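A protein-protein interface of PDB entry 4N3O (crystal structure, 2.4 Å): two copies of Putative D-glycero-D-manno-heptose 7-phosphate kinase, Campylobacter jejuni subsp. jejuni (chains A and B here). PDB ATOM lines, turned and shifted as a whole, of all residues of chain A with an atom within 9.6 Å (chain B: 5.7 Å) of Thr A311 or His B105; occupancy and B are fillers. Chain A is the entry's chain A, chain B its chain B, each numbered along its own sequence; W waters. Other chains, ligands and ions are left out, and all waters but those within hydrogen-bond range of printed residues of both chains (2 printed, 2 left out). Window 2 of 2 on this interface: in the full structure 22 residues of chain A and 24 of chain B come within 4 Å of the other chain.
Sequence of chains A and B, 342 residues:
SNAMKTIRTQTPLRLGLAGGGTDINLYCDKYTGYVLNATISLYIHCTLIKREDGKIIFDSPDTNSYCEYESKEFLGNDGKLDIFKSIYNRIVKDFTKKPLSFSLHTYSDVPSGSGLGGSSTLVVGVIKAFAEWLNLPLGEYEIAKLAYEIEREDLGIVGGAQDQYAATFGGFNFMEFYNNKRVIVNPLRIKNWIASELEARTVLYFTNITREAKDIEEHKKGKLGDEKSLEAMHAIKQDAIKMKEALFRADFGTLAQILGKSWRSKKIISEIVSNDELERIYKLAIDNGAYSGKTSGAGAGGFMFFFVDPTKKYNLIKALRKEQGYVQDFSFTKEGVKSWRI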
ATOM      1  N   GLU A 197      17.421  14.741   6.834  1.00  0.00           N
ATOM      2  CA  GLU A 197      16.428  13.691   6.624  1.00  0.00           C
ATOM      3  C   GLU A 197      15.160  14.331   6.084  1.00  0.00           C
ATOM      4  O   GLU A 197      14.530  13.800   5.167  1.00  0.00           O
ATOM      5  CB  GLU A 197      16.147  12.923   7.916  1.00  0.00           C
ATOM      6  CG  GLU A 197      15.110  11.825   7.750  1.00  0.00           C
ATOM      7  CD  GLU A 197      15.573  10.704   6.831  1.00  0.00           C
ATOM      8  OE1 GLU A 197      16.796  10.566   6.605  1.00  0.00           O
ATOM      9  OE2 GLU A 197      14.721   9.936   6.351  1.00  0.00           O
ATOM     10  N   ALA A 200      15.694  15.006   2.515  1.00  0.00           N
ATOM     11  CA  ALA A 200      15.663  13.752   1.726  1.00  0.00           C
ATOM     12  C   ALA A 200      14.231  13.301   1.441  1.00  0.00           C
ATOM     13  O   ALA A 200      13.971  12.669   0.412  1.00  0.00           O
ATOM     14  CB  ALA A 200      16.426  12.652   2.443  1.00  0.00           C
ATOM     15  N   ARG A 201      13.312  13.661   2.344  1.00  0.00           N
ATOM     16  CA  ARG A 201      11.898  13.305   2.239  1.00  0.00           C
ATOM     17  C   ARG A 201      11.053  14.352   1.549  1.00  0.00           C
ATOM     18  O   ARG A 201       9.850  14.206   1.507  1.00  0.00           O
ATOM     19  CB  ARG A 201      11.267  13.256   3.630  1.00  0.00           C
ATOM     20  CG  ARG A 201      11.932  12.435   4.704  1.00  0.00           C
ATOM     21  CD  ARG A 201      11.405  11.049   4.796  1.00  0.00           C
ATOM     22  NE  ARG A 201      11.776  10.473   6.075  1.00  0.00           N
ATOM     23  CZ  ARG A 201      11.464   9.240   6.444  1.00  0.00           C
ATOM     24  NH1 ARG A 201      11.852   8.786   7.628  1.00  0.00           N
ATOM     25  NH2 ARG A 201      10.780   8.452   5.617  1.00  0.00           N
ATOM     26  N   THR A 202      11.617  15.427   1.039  1.00  0.00           N
ATOM     27  CA  THR A 202      10.735  16.444   0.522  1.00  0.00           C
ATOM     28  C   THR A 202      11.049  16.978  -0.865  1.00  0.00           C
ATOM     29  O   THR A 202      12.188  17.023  -1.291  1.00  0.00           O
ATOM     30  CB  THR A 202      10.623  17.638   1.532  1.00  0.00           C
ATOM     31  OG1 THR A 202      11.898  18.199   1.802  1.00  0.00           O
ATOM     32  CG2 THR A 202      10.036  17.190   2.857  1.00  0.00           C
ATOM     33  N   ASN A 288       3.222   8.726  -7.831  1.00  0.00           N
ATOM     34  CA  ASN A 288       4.653   8.560  -8.028  1.00  0.00           C
ATOM     35  C   ASN A 288       5.517   8.551  -6.786  1.00  0.00           C
ATOM     36  O   ASN A 288       6.704   8.844  -6.870  1.00  0.00           O
ATOM     37  CB  ASN A 288       5.147   9.651  -8.973  1.00  0.00           C
ATOM     38  CG  ASN A 288       4.804   9.370 -10.410  1.00  0.00           C
ATOM     39  OD1 ASN A 288       5.421   8.520 -11.039  1.00  0.00           O
ATOM     40  ND2 ASN A 288       3.870  10.127 -10.961  1.00  0.00           N
ATOM     41  N   GLY A 289       4.964   8.226  -5.634  1.00  0.00           N
ATOM     42  CA  GLY A 289       5.838   8.153  -4.463  1.00  0.00           C
ATOM     43  C   GLY A 289       5.546   9.090  -3.322  1.00  0.00           C
ATOM     44  O   GLY A 289       5.886   8.784  -2.181  1.00  0.00           O
ATOM     45  N   ALA A 290       4.938  10.236  -3.596  1.00  0.00           N
ATOM     46  CA  ALA A 290       4.589  11.146  -2.505  1.00  0.00           C
ATOM     47  C   ALA A 290       3.507  10.476  -1.660  1.00  0.00           C
ATOM     48  O   ALA A 290       2.702   9.700  -2.186  1.00  0.00           O
ATOM     49  CB  ALA A 290       4.091  12.482  -3.040  1.00  0.00           C
ATOM     50  N   TYR A 291       3.519  10.738  -0.357  1.00  0.00           N
ATOM     51  CA  TYR A 291       2.497  10.193   0.546  1.00  0.00           C
ATOM     52  C   TYR A 291       1.795  11.300   1.310  1.00  0.00           C
ATOM     53  O   TYR A 291       0.953  11.042   2.162  1.00  0.00           O
ATOM     54  CB  TYR A 291       3.085   9.157   1.519  1.00  0.00           C
ATOM     55  CG  TYR A 291       4.227   9.632   2.394  1.00  0.00           C
ATOM     56  CD1 TYR A 291       3.992  10.323   3.589  1.00  0.00           C
ATOM     57  CD2 TYR A 291       5.545   9.348   2.054  1.00  0.00           C
ATOM     58  CE1 TYR A 291       5.040  10.741   4.400  1.00  0.00           C
ATOM     59  CE2 TYR A 291       6.601   9.760   2.857  1.00  0.00           C
ATOM     60  CZ  TYR A 291       6.349  10.455   4.030  1.00  0.00           C
ATOM     61  OH  TYR A 291       7.418  10.855   4.814  1.00  0.00           O
ATOM     62  N   VAL A 308       7.906  12.486   0.541  1.00  0.00           N
ATOM     63  CA  VAL A 308       8.097  11.315  -0.295  1.00  0.00           C
ATOM     64  C   VAL A 308       9.145  10.382   0.280  1.00  0.00           C
ATOM     65  O   VAL A 308      10.025  10.781   1.035  1.00  0.00           O
ATOM     66  CB  VAL A 308       8.589  11.730  -1.695  1.00  0.00           C
ATOM     67  CG1 VAL A 308       9.976  12.357  -1.616  1.00  0.00           C
ATOM     68  CG2 VAL A 308       8.605  10.543  -2.644  1.00  0.00           C
ATOM     69  N   ASP A 309       9.031   9.124  -0.071  1.00  0.00           N
ATOM     70  CA  ASP A 309      10.018   8.169   0.329  1.00  0.00           C
ATOM     71  C   ASP A 309      11.293   8.538  -0.454  1.00  0.00           C
ATOM     72  O   ASP A 309      11.250   8.708  -1.681  1.00  0.00           O
ATOM     73  CB  ASP A 309       9.541   6.784  -0.047  1.00  0.00           C
ATOM     74  CG  ASP A 309      10.561   5.731   0.216  1.00  0.00           C
ATOM     75  OD1 ASP A 309      11.335   5.847   1.189  1.00  0.00           O
ATOM     76  OD2 ASP A 309      10.561   4.757  -0.554  1.00  0.00           O
ATOM     77  N   PRO A 310      12.418   8.686   0.244  1.00  0.00           N
ATOM     78  CA  PRO A 310      13.650   9.033  -0.452  1.00  0.00           C
ATOM     79  C   PRO A 310      14.012   8.094  -1.601  1.00  0.00           C
ATOM     80  O   PRO A 310      14.511   8.546  -2.615  1.00  0.00           O
ATOM     81  CB  PRO A 310      14.689   8.969   0.652  1.00  0.00           C
ATOM     82  CG  PRO A 310      13.909   9.352   1.882  1.00  0.00           C
ATOM     83  CD  PRO A 310      12.593   8.663   1.704  1.00  0.00           C
ATOM     84  N   THR A 311      13.734   6.805  -1.481  1.00  0.00           N
ATOM     85  CA  THR A 311      14.047   5.893  -2.594  1.00  0.00           C
ATOM     86  C   THR A 311      13.091   6.057  -3.778  1.00  0.00           C
ATOM     87  O   THR A 311      13.188   5.323  -4.755  1.00  0.00           O
ATOM     88  CB  THR A 311      14.022   4.426  -2.155  1.00  0.00           C
ATOM     89  OG1 THR A 311      12.683   4.037  -1.856  1.00  0.00           O
ATOM     90  CG2 THR A 311      14.890   4.221  -0.940  1.00  0.00           C
ATOM     91  N   LYS A 312      12.162   7.003  -3.684  1.00  0.00           N
ATOM     92  CA  LYS A 312      11.191   7.241  -4.759  1.00  0.00           C
ATOM     93  C   LYS A 312      11.251   8.679  -5.242  1.00  0.00           C
ATOM     94  O   LYS A 312      10.609   9.037  -6.229  1.00  0.00           O
ATOM     95  CB  LYS A 312       9.785   7.036  -4.222  1.00  0.00           C
ATOM     96  CG  LYS A 312       9.452   5.667  -3.657  1.00  0.00           C
ATOM     97  CD  LYS A 312       8.805   4.750  -4.664  1.00  0.00           C
ATOM     98  CE  LYS A 312       8.099   3.618  -3.921  1.00  0.00           C
ATOM     99  NZ  LYS A 312       7.293   2.753  -4.819  1.00  0.00           N
ATOM    100  N   LYS A 313      12.024   9.502  -4.546  1.00  0.00           N
ATOM    101  CA  LYS A 313      12.073  10.924  -4.847  1.00  0.00           C
ATOM    102  C   LYS A 313      12.539  11.242  -6.255  1.00  0.00           C
ATOM    103  O   LYS A 313      12.029  12.174  -6.873  1.00  0.00           O
ATOM    104  CB  LYS A 313      12.940  11.641  -3.813  1.00  0.00           C
ATOM    105  CG  LYS A 313      13.144  13.112  -4.066  1.00  0.00           C
ATOM    106  CD  LYS A 313      13.743  13.778  -2.837  1.00  0.00           C
ATOM    107  CE  LYS A 313      14.126  15.213  -3.113  1.00  0.00           C
ATOM    108  NZ  LYS A 313      14.750  15.836  -1.915  1.00  0.00           N
ATOM    109  N   TYR A 314      13.498  10.477  -6.775  1.00  0.00           N
ATOM    110  CA  TYR A 314      13.991  10.793  -8.106  1.00  0.00           C
ATOM    111  C   TYR A 314      12.888  10.625  -9.146  1.00  0.00           C
ATOM    112  O   TYR A 314      12.710  11.499 -10.001  1.00  0.00           O
ATOM    113  CB  TYR A 314      15.210   9.976  -8.489  1.00  0.00           C
ATOM    114  CG  TYR A 314      15.648  10.278  -9.891  1.00  0.00           C
ATOM    115  CD1 TYR A 314      16.415  11.400 -10.177  1.00  0.00           C
ATOM    116  CD2 TYR A 314      15.261   9.472 -10.938  1.00  0.00           C
ATOM    117  CE1 TYR A 314      16.803  11.694 -11.478  1.00  0.00           C
ATOM    118  CE2 TYR A 314      15.637   9.755 -12.236  1.00  0.00           C
ATOM    119  CZ  TYR A 314      16.413  10.867 -12.501  1.00  0.00           C
ATOM    120  OH  TYR A 314      16.788  11.129 -13.811  1.00  0.00           O
ATOM    121  N   ASN A 315      12.162   9.502  -9.075  1.00  0.00           N
ATOM    122  CA  ASN A 315      11.080   9.257 -10.013  1.00  0.00           C
ATOM    123  C   ASN A 315       9.940  10.292  -9.844  1.00  0.00           C
ATOM    124  O   ASN A 315       9.316  10.665 -10.803  1.00  0.00           O
ATOM    125  CB  ASN A 315      10.586   7.794  -9.963  1.00  0.00           C
ATOM    126  CG  ASN A 315      11.566   6.811 -10.642  1.00  0.00           C
ATOM    127  OD1 ASN A 315      12.111   7.084 -11.723  1.00  0.00           O
ATOM    128  ND2 ASN A 315      11.783   5.651 -10.007  1.00  0.00           N
ATOM    129  N   LEU A 316       9.694  10.757  -8.636  1.00  0.00           N
ATOM    130  CA  LEU A 316       8.687  11.800  -8.428  1.00  0.00           C
ATOM    131  C   LEU A 316       9.138  13.085  -9.127  1.00  0.00           C
ATOM    132  O   LEU A 316       8.386  13.696  -9.877  1.00  0.00           O
ATOM    133  CB  LEU A 316       8.471  12.045  -6.944  1.00  0.00           C
ATOM    134  CG  LEU A 316       7.602  13.231  -6.533  1.00  0.00           C
ATOM    135  CD1 LEU A 316       6.287  13.270  -7.287  1.00  0.00           C
ATOM    136  CD2 LEU A 316       7.378  13.144  -5.027  1.00  0.00           C
ATOM    137  N   ILE A 317      10.384  13.469  -8.895  1.00  0.00           N
ATOM    138  CA  ILE A 317      10.951  14.652  -9.524  1.00  0.00           C
ATOM    139  C   ILE A 317      10.863  14.522 -11.050  1.00  0.00           C
ATOM    140  O   ILE A 317      10.477  15.458 -11.744  1.00  0.00           O
ATOM    141  CB  ILE A 317      12.396  14.867  -9.058  1.00  0.00           C
ATOM    142  CG1 ILE A 317      12.393  15.294  -7.594  1.00  0.00           C
ATOM    143  CG2 ILE A 317      13.080  15.945  -9.870  1.00  0.00           C
ATOM    144  CD1 ILE A 317      13.766  15.500  -6.997  1.00  0.00           C
ATOM    145  N   ARG B   8      21.854   6.674   5.270  1.00  0.00           N
ATOM    146  CA  ARG B   8      21.807   7.558   4.112  1.00  0.00           C
ATOM    147  C   ARG B   8      23.082   8.324   4.086  1.00  0.00           C
ATOM    148  O   ARG B   8      23.659   8.583   5.132  1.00  0.00           O
ATOM    149  CB  ARG B   8      20.645   8.577   4.153  1.00  0.00           C
ATOM    150  CG  ARG B   8      19.245   7.982   4.278  1.00  0.00           C
ATOM    151  CD  ARG B   8      18.165   8.981   3.905  1.00  0.00           C
ATOM    152  NE  ARG B   8      16.908   8.656   4.577  1.00  0.00           N
ATOM    153  CZ  ARG B   8      16.031   7.736   4.174  1.00  0.00           C
ATOM    154  NH1 ARG B   8      14.943   7.525   4.896  1.00  0.00           N
ATOM    155  NH2 ARG B   8      16.229   7.010   3.081  1.00  0.00           N
ATOM    156  N   HIS B  45      22.944  11.316  -3.698  1.00  0.00           N
ATOM    157  CA  HIS B  45      22.249  10.817  -2.532  1.00  0.00           C
ATOM    158  C   HIS B  45      22.202   9.321  -2.562  1.00  0.00           C
ATOM    159  O   HIS B  45      21.867   8.746  -3.582  1.00  0.00           O
ATOM    160  CB  HIS B  45      20.801  11.312  -2.545  1.00  0.00           C
ATOM    161  CG  HIS B  45      20.661  12.779  -2.826  1.00  0.00           C
ATOM    162  ND1 HIS B  45      20.650  13.729  -1.832  1.00  0.00           N
ATOM    163  CD2 HIS B  45      20.538  13.455  -3.991  1.00  0.00           C
ATOM    164  CE1 HIS B  45      20.530  14.932  -2.371  1.00  0.00           C
ATOM    165  NE2 HIS B  45      20.461  14.793  -3.681  1.00  0.00           N
ATOM    166  N   CYS B  46      22.545   8.679  -1.446  1.00  0.00           N
ATOM    167  CA  CYS B  46      22.465   7.230  -1.338  1.00  0.00           C
ATOM    168  C   CYS B  46      21.624   6.826  -0.142  1.00  0.00           C
ATOM    169  O   CYS B  46      21.659   7.477   0.899  1.00  0.00           O
ATOM    170  CB  CYS B  46      23.848   6.597  -1.134  1.00  0.00           C
ATOM    171  SG  CYS B  46      25.047   6.871  -2.442  1.00  0.00           S
ATOM    172  N   THR B  47      20.894   5.730  -0.301  1.00  0.00           N
ATOM    173  CA  THR B  47      20.116   5.110   0.783  1.00  0.00           C
ATOM    174  C   THR B  47      20.451   3.601   0.763  1.00  0.00           C
ATOM    175  O   THR B  47      20.410   2.969  -0.290  1.00  0.00           O
ATOM    176  CB  THR B  47      18.605   5.327   0.646  1.00  0.00           C
ATOM    177  OG1 THR B  47      18.275   6.664   1.042  1.00  0.00           O
ATOM    178  CG2 THR B  47      17.833   4.382   1.526  1.00  0.00           C
ATOM    179  N   LEU B  48      20.813   3.048   1.920  1.00  0.00           N
ATOM    180  CA  LEU B  48      21.161   1.630   2.041  1.00  0.00           C
ATOM    181  C   LEU B  48      20.270   1.035   3.122  1.00  0.00           C
ATOM    182  O   LEU B  48      20.243   1.527   4.254  1.00  0.00           O
ATOM    183  CB  LEU B  48      22.641   1.457   2.403  1.00  0.00           C
ATOM    184  CG  LEU B  48      23.242   0.039   2.374  1.00  0.00           C
ATOM    185  CD1 LEU B  48      24.740   0.074   2.493  1.00  0.00           C
ATOM    186  CD2 LEU B  48      22.674  -0.851   3.477  1.00  0.00           C
ATOM    187  N   ILE B  49      19.542  -0.018   2.775  1.00  0.00           N
ATOM    188  CA  ILE B  49      18.607  -0.629   3.707  1.00  0.00           C
ATOM    189  C   ILE B  49      18.925  -2.092   3.928  1.00  0.00           C
ATOM    190  O   ILE B  49      18.990  -2.871   2.974  1.00  0.00           O
ATOM    191  CB  ILE B  49      17.165  -0.551   3.176  1.00  0.00           C
ATOM    192  CG1 ILE B  49      16.836   0.875   2.712  1.00  0.00           C
ATOM    193  CG2 ILE B  49      16.183  -1.001   4.258  1.00  0.00           C
ATOM    194  CD1 ILE B  49      15.480   0.994   2.037  1.00  0.00           C
ATOM    195  N   ILE B  57      20.113  -5.700  -3.755  1.00  0.00           N
ATOM    196  CA  ILE B  57      19.482  -4.893  -4.798  1.00  0.00           C
ATOM    197  C   ILE B  57      20.258  -3.608  -5.026  1.00  0.00           C
ATOM    198  O   ILE B  57      20.617  -2.938  -4.072  1.00  0.00           O
ATOM    199  CB  ILE B  57      18.012  -4.569  -4.418  1.00  0.00           C
ATOM    200  CG1 ILE B  57      17.179  -5.863  -4.457  1.00  0.00           C
ATOM    201  CG2 ILE B  57      17.414  -3.488  -5.335  1.00  0.00           C
ATOM    202  CD1 ILE B  57      15.721  -5.671  -4.104  1.00  0.00           C
ATOM    203  N   ASP B  59      19.781  -0.107  -7.072  1.00  0.00           N
ATOM    204  CA  ASP B  59      18.750   0.688  -7.757  1.00  0.00           C
ATOM    205  C   ASP B  59      19.284   2.100  -8.031  1.00  0.00           C
ATOM    206  O   ASP B  59      19.501   2.886  -7.110  1.00  0.00           O
ATOM    207  CB  ASP B  59      17.498   0.705  -6.866  1.00  0.00           C
ATOM    208  CG  ASP B  59      16.362   1.591  -7.404  1.00  0.00           C
ATOM    209  OD1 ASP B  59      16.252   1.837  -8.630  1.00  0.00           O
ATOM    210  OD2 ASP B  59      15.535   2.022  -6.564  1.00  0.00           O
ATOM    211  N   SER B  60      19.515   2.405  -9.300  1.00  0.00           N
ATOM    212  CA  SER B  60      20.029   3.716  -9.709  1.00  0.00           C
ATOM    213  C   SER B  60      19.143   4.220 -10.848  1.00  0.00           C
ATOM    214  O   SER B  60      19.482   4.096 -12.043  1.00  0.00           O
ATOM    215  CB  SER B  60      21.500   3.615 -10.106  1.00  0.00           C
ATOM    216  OG  SER B  60      21.866   4.681 -10.963  1.00  0.00           O
ATOM    217  N   PRO B  61      17.984   4.790 -10.482  1.00  0.00           N
ATOM    218  CA  PRO B  61      16.992   5.217 -11.475  1.00  0.00           C
ATOM    219  C   PRO B  61      17.447   6.343 -12.402  1.00  0.00           C
ATOM    220  O   PRO B  61      16.966   6.433 -13.543  1.00  0.00           O
ATOM    221  CB  PRO B  61      15.811   5.660 -10.617  1.00  0.00           C
ATOM    222  CG  PRO B  61      16.420   6.067  -9.323  1.00  0.00           C
ATOM    223  CD  PRO B  61      17.588   5.146  -9.112  1.00  0.00           C
ATOM    224  N   SER B 103      19.529  -3.355   0.200  1.00  0.00           N
ATOM    225  CA  SER B 103      19.165  -2.616  -1.024  1.00  0.00           C
ATOM    226  C   SER B 103      19.928  -1.282  -1.003  1.00  0.00           C
ATOM    227  O   SER B 103      20.039  -0.639   0.027  1.00  0.00           O
ATOM    228  CB  SER B 103      17.654  -2.382  -1.155  1.00  0.00           C
ATOM    229  OG  SER B 103      17.124  -1.558  -0.130  1.00  0.00           O
ATOM    230  N   LEU B 104      20.486  -0.903  -2.139  1.00  0.00           N
ATOM    231  CA  LEU B 104      21.258   0.307  -2.276  1.00  0.00           C
ATOM    232  C   LEU B 104      20.561   1.112  -3.359  1.00  0.00           C
ATOM    233  O   LEU B 104      20.299   0.588  -4.440  1.00  0.00           O
ATOM    234  CB  LEU B 104      22.696  -0.047  -2.667  1.00  0.00           C
ATOM    235  CG  LEU B 104      23.694   1.089  -2.926  1.00  0.00           C
ATOM    236  CD1 LEU B 104      23.916   1.904  -1.667  1.00  0.00           C
ATOM    237  CD2 LEU B 104      25.011   0.517  -3.428  1.00  0.00           C
ATOM    238  N   HIS B 105      20.257   2.374  -3.069  1.00  0.00           N
ATOM    239  CA  HIS B 105      19.476   3.235  -3.978  1.00  0.00           C
ATOM    240  C   HIS B 105      20.198   4.548  -4.127  1.00  0.00           C
ATOM    241  O   HIS B 105      20.571   5.109  -3.135  1.00  0.00           O
ATOM    242  CB  HIS B 105      18.103   3.525  -3.377  1.00  0.00           C
ATOM    243  CG  HIS B 105      17.398   2.314  -2.852  1.00  0.00           C
ATOM    244  ND1 HIS B 105      16.431   1.643  -3.569  1.00  0.00           N
ATOM    245  CD2 HIS B 105      17.512   1.662  -1.673  1.00  0.00           C
ATOM    246  CE1 HIS B 105      15.967   0.640  -2.848  1.00  0.00           C
ATOM    247  NE2 HIS B 105      16.613   0.621  -1.700  1.00  0.00           N
ATOM    248  N   THR B 106      20.361   5.058  -5.345  1.00  0.00           N
ATOM    249  CA  THR B 106      21.127   6.272  -5.515  1.00  0.00           C
ATOM    250  C   THR B 106      20.684   7.118  -6.672  1.00  0.00           C
ATOM    251  O   THR B 106      20.157   6.616  -7.648  1.00  0.00           O
ATOM    252  CB  THR B 106      22.609   5.950  -5.816  1.00  0.00           C
ATOM    253  OG1 THR B 106      22.736   5.337  -7.115  1.00  0.00           O
ATOM    254  CG2 THR B 106      23.193   5.050  -4.778  1.00  0.00           C
ATOM    255  N   TYR B 107      20.894   8.425  -6.550  1.00  0.00           N
ATOM    256  CA  TYR B 107      20.632   9.325  -7.664  1.00  0.00           C
ATOM    257  C   TYR B 107      21.465  10.567  -7.455  1.00  0.00           C
ATOM    258  O   TYR B 107      21.873  10.887  -6.320  1.00  0.00           O
ATOM    259  CB  TYR B 107      19.139   9.654  -7.832  1.00  0.00           C
ATOM    260  CG  TYR B 107      18.574  10.647  -6.862  1.00  0.00           C
ATOM    261  CD1 TYR B 107      18.172  10.257  -5.590  1.00  0.00           C
ATOM    262  CD2 TYR B 107      18.433  11.978  -7.211  1.00  0.00           C
ATOM    263  CE1 TYR B 107      17.660  11.172  -4.685  1.00  0.00           C
ATOM    264  CE2 TYR B 107      17.924  12.904  -6.309  1.00  0.00           C
ATOM    265  CZ  TYR B 107      17.543  12.488  -5.046  1.00  0.00           C
ATOM    266  OH  TYR B 107      17.040  13.380  -4.146  1.00  0.00           O
HETATM  267  O   HOH W   1      14.314   5.124   2.750  1.00  0.00           O
HETATM  268  O   HOH W   2      15.694   4.571  -5.712  1.00  0.00           O
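The backbone carbonyl oxygen of Thr A202 lies within hydrogen-bond range of the side-chain amino group of Lys A313 (2.9 Å).
OG of Ser B103 is in hydrogen-bond range of NE2 of His B105, 2.7 Å away.
The backbone NH of His B45 sits at hydrogen-bond distance from the backbone carbonyl oxygen of Tyr B107 (2.9 Å).
The side-chain hydroxyl (OG1) of Thr B47 lies within hydrogen-bond range of the guanidinium group (NH2) of Arg B8, 2.9 Å away.
The backbone carbonyl oxygen (O) of Thr B47 lies within hydrogen-bond range of the backbone NH (N) of His B105 (2.8 Å).
ND1 of His B105 sits at hydrogen-bond distance from OD2 of Asp B59 (3.1 Å).
Of the 15 printed residues of chain B, 5 touch a printed residue of chain A.
Hydrophobic or aromatic side chains of chain B that line the printed part of chain A: Pro B61, His B105 and Tyr B107.
Among the printed residues, 7 pairs touch across the chains.
Thr A311 touches two residues of chain B.
Of chain A, only Thr A311 comes within 4 Å of His B105.
Of chain A, only Thr A311 (3.8 Å) comes within 4 Å of Thr B47.
No residue of chain A comes within 4 Å of Ser B103.
No residue of chain A comes within 4 Å of Leu B104.
No residue of chain A comes within 4 Å of Thr B106.
Printed residues of chain A within 4 Å of Arg B8: Glu A197 and Pro A310.
Of the printed residues of chain B, Tyr A314 touches Pro B61 (3.8 Å) and Tyr B107 (3.6 Å).
Of the printed residues of chain B, Pro A310 touches Arg B8.
Of the printed residues of chain A, Tyr B107 touches Lys A313 and Tyr A314.
Printed residues of chain B within 4 Å of Glu A197: Arg B8.
Ala A290 touches none of the printed residues of chain B.
OE1 of Glu A197 is in salt-bridge range of NE of Arg B8, at 2.8 Å.
No position is printed for both chains.
Water W2 lies within hydrogen-bond range of the side-chain carboxylate (OD2) of Asp B59 (2.7 Å) and the backbone carbonyl oxygen (O) of Thr A311 (2.8 Å).
Water W1 bridges the guanidinium group of Arg B8 (2.7 Å) and the side-chain carboxylate of Asp A309 (3.4 Å).
Among the printed residues, pairs that only touch across the chains: Pro A310 with Arg B8, Thr A311 with Thr B47, Thr A311 with His B105, Lys A313 with Tyr B107, Tyr A314 with Pro B61 and Tyr A314 with Tyr B107.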
